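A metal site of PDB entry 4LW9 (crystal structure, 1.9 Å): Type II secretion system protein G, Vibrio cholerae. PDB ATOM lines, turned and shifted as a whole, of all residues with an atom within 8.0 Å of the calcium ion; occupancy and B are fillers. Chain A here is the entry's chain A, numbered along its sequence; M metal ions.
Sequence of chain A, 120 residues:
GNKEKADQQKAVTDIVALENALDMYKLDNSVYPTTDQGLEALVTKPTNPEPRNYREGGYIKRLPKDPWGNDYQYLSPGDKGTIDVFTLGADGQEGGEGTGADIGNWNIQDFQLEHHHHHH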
ATOM      1  N   THR A  87      24.912 -22.151   8.221  1.00  0.00           N
ATOM      2  CA  THR A  87      24.463 -22.608   9.518  1.00  0.00           C
ATOM      3  C   THR A  87      25.274 -21.908  10.620  1.00  0.00           C
ATOM      4  O   THR A  87      26.475 -21.637  10.461  1.00  0.00           O
ATOM      5  CB  THR A  87      24.590 -24.111   9.708  1.00  0.00           C
ATOM      6  OG1 THR A  87      24.319 -24.398  11.086  1.00  0.00           O
ATOM      7  CG2 THR A  87      26.017 -24.633   9.376  1.00  0.00           C
ATOM      8  N   LEU A  88      24.598 -21.627  11.731  1.00  0.00           N
ATOM      9  CA  LEU A  88      25.246 -20.976  12.872  1.00  0.00           C
ATOM     10  C   LEU A  88      25.898 -21.981  13.830  1.00  0.00           C
ATOM     11  O   LEU A  88      26.506 -21.581  14.832  1.00  0.00           O
ATOM     12  CB  LEU A  88      24.244 -20.078  13.619  1.00  0.00           C
ATOM     13  CG  LEU A  88      23.837 -18.793  12.896  1.00  0.00           C
ATOM     14  CD1 LEU A  88      22.923 -17.956  13.782  1.00  0.00           C
ATOM     15  CD2 LEU A  88      25.045 -17.961  12.499  1.00  0.00           C
ATOM     16  N   GLY A  89      25.806 -23.269  13.522  1.00  0.00           N
ATOM     17  CA  GLY A  89      26.569 -24.285  14.233  1.00  0.00           C
ATOM     18  C   GLY A  89      25.887 -24.802  15.483  1.00  0.00           C
ATOM     19  O   GLY A  89      24.683 -24.579  15.692  1.00  0.00           O
ATOM     20  N   ALA A  90      26.653 -25.496  16.324  1.00  0.00           N
ATOM     21  CA  ALA A  90      26.123 -26.165  17.507  1.00  0.00           C
ATOM     22  C   ALA A  90      25.468 -25.217  18.534  1.00  0.00           C
ATOM     23  O   ALA A  90      24.525 -25.600  19.219  1.00  0.00           O
ATOM     24  CB  ALA A  90      27.232 -26.980  18.200  1.00  0.00           C
ATOM     25  N   ASP A  91      25.948 -23.991  18.629  1.00  0.00           N
ATOM     26  CA  ASP A  91      25.415 -23.064  19.630  1.00  0.00           C
ATOM     27  C   ASP A  91      24.194 -22.286  19.129  1.00  0.00           C
ATOM     28  O   ASP A  91      23.576 -21.540  19.883  1.00  0.00           O
ATOM     29  CB  ASP A  91      26.495 -22.085  20.123  1.00  0.00           C
ATOM     30  CG  ASP A  91      27.138 -21.298  19.002  1.00  0.00           C
ATOM     31  OD1 ASP A  91      26.641 -21.349  17.844  1.00  0.00           O
ATOM     32  OD2 ASP A  91      28.154 -20.623  19.275  1.00  0.00           O
ATOM     33  N   GLY A  92      23.862 -22.455  17.848  1.00  0.00           N
ATOM     34  CA  GLY A  92      22.717 -21.774  17.260  1.00  0.00           C
ATOM     35  C   GLY A  92      22.797 -20.261  17.315  1.00  0.00           C
ATOM     36  O   GLY A  92      21.785 -19.589  17.311  1.00  0.00           O
ATOM     37  N   GLN A  93      24.010 -19.717  17.358  1.00  0.00           N
ATOM     38  CA  GLN A  93      24.219 -18.281  17.537  1.00  0.00           C
ATOM     39  C   GLN A  93      25.353 -17.801  16.628  1.00  0.00           C
ATOM     40  O   GLN A  93      26.157 -18.597  16.180  1.00  0.00           O
ATOM     41  CB  GLN A  93      24.501 -17.983  19.026  1.00  0.00           C
ATOM     42  CG  GLN A  93      25.697 -17.088  19.299  1.00  0.00           C
ATOM     43  CD  GLN A  93      25.882 -16.756  20.777  1.00  0.00           C
ATOM     44  OE1 GLN A  93      25.697 -15.611  21.193  1.00  0.00           O
ATOM     45  NE2 GLN A  93      26.278 -17.747  21.571  1.00  0.00           N
ATOM     46  N   GLU A  94      25.380 -16.500  16.342  1.00  0.00           N
ATOM     47  CA  GLU A  94      26.448 -15.892  15.565  1.00  0.00           C
ATOM     48  C   GLU A  94      27.798 -16.059  16.270  1.00  0.00           C
ATOM     49  O   GLU A  94      27.874 -16.033  17.505  1.00  0.00           O
ATOM     50  CB  GLU A  94      26.140 -14.408  15.377  1.00  0.00           C
ATOM     51  CG  GLU A  94      26.696 -13.759  14.116  1.00  0.00           C
ATOM     52  CD  GLU A  94      25.921 -12.515  13.742  1.00  0.00           C
ATOM     53  OE1 GLU A  94      24.678 -12.533  13.892  1.00  0.00           O
ATOM     54  OE2 GLU A  94      26.543 -11.518  13.288  1.00  0.00           O
ATOM     55  N   GLY A  95      28.873 -16.251  15.500  1.00  0.00           N
ATOM     56  CA  GLY A  95      30.197 -16.518  16.068  1.00  0.00           C
ATOM     57  C   GLY A  95      30.292 -17.799  16.877  1.00  0.00           C
ATOM     58  O   GLY A  95      29.347 -18.577  16.963  1.00  0.00           O
ATOM     59  N   GLY A  96      31.459 -18.021  17.471  1.00  0.00           N
ATOM     60  CA  GLY A  96      31.703 -19.218  18.277  1.00  0.00           C
ATOM     61  C   GLY A  96      32.862 -20.019  17.728  1.00  0.00           C
ATOM     62  O   GLY A  96      33.247 -19.852  16.572  1.00  0.00           O
ATOM     63  N   GLU A  97      33.424 -20.887  18.570  1.00  0.00           N
ATOM     64  CA  GLU A  97      34.518 -21.760  18.151  1.00  0.00           C
ATOM     65  C   GLU A  97      34.100 -23.215  18.337  1.00  0.00           C
ATOM     66  O   GLU A  97      33.065 -23.499  18.931  1.00  0.00           O
ATOM     67  CB  GLU A  97      35.792 -21.478  18.954  1.00  0.00           C
ATOM     68  N   GLY A  98      34.935 -24.123  17.836  1.00  0.00           N
ATOM     69  CA  GLY A  98      34.635 -25.543  17.894  1.00  0.00           C
ATOM     70  C   GLY A  98      33.423 -25.841  17.046  1.00  0.00           C
ATOM     71  O   GLY A  98      33.242 -25.240  15.990  1.00  0.00           O
ATOM     72  N   THR A  99      32.579 -26.754  17.519  1.00  0.00           N
ATOM     73  CA  THR A  99      31.324 -27.096  16.836  1.00  0.00           C
ATOM     74  C   THR A  99      30.362 -25.919  16.790  1.00  0.00           C
ATOM     75  O   THR A  99      29.378 -25.922  16.051  1.00  0.00           O
ATOM     76  CB  THR A  99      30.635 -28.299  17.521  1.00  0.00           C
ATOM     77  OG1 THR A  99      30.391 -27.984  18.885  1.00  0.00           O
ATOM     78  CG2 THR A  99      31.501 -29.550  17.443  1.00  0.00           C
ATOM     79  N   GLY A 100      30.653 -24.894  17.586  1.00  0.00           N
ATOM     80  CA  GLY A 100      29.868 -23.682  17.576  1.00  0.00           C
ATOM     81  C   GLY A 100      30.148 -22.766  16.421  1.00  0.00           C
ATOM     82  O   GLY A 100      29.369 -21.867  16.166  1.00  0.00           O
ATOM     83  N   ALA A 101      31.224 -22.979  15.678  1.00  0.00           N
ATOM     84  CA  ALA A 101      31.544 -22.064  14.595  1.00  0.00           C
ATOM     85  C   ALA A 101      30.520 -22.091  13.478  1.00  0.00           C
ATOM     86  O   ALA A 101      29.892 -23.125  13.203  1.00  0.00           O
ATOM     87  CB  ALA A 101      32.917 -22.320  14.021  1.00  0.00           C
ATOM     88  N   ASP A 102      30.364 -20.925  12.865  1.00  0.00           N
ATOM     89  CA  ASP A 102      29.427 -20.680  11.774  1.00  0.00           C
ATOM     90  C   ASP A 102      30.048 -21.165  10.489  1.00  0.00           C
ATOM     91  O   ASP A 102      31.197 -20.860  10.183  1.00  0.00           O
ATOM     92  CB  ASP A 102      29.140 -19.186  11.634  1.00  0.00           C
ATOM     93  CG  ASP A 102      28.591 -18.554  12.926  1.00  0.00           C
ATOM     94  OD1 ASP A 102      28.046 -19.262  13.798  1.00  0.00           O
ATOM     95  OD2 ASP A 102      28.733 -17.325  13.040  1.00  0.00           O
ATOM     96  N   ILE A 103      29.270 -21.942   9.718  1.00  0.00           N
ATOM     97  CA  ILE A 103      29.736 -22.471   8.471  1.00  0.00           C
ATOM     98  C   ILE A 103      28.860 -21.911   7.357  1.00  0.00           C
ATOM     99  O   ILE A 103      27.641 -22.076   7.416  1.00  0.00           O
ATOM    100  CB  ILE A 103      29.647 -24.024   8.477  1.00  0.00           C
ATOM    101  CG1 ILE A 103      30.357 -24.617   9.704  1.00  0.00           C
ATOM    102  CG2 ILE A 103      30.150 -24.551   7.139  1.00  0.00           C
ATOM    103  CD1 ILE A 103      30.194 -26.101   9.916  1.00  0.00           C
HETATM  104 CA    CA M   1      27.907 -20.098  15.949  1.00  0.00          CA
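Of the 17 residues printed, 6 come within 4 Å of the calcium ion.
The calcium ion is bound by O of Gly 100 (2.3 Å), OD1 of Asp 102 (2.3 Å), O of Gln 93 (2.3 Å), O of Leu 88 (2.3 Å), O of Gly 95 (2.3 Å) and OD1 of Asp 91 (2.6 Å). The calcium ion has six donor atoms within binding distance.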
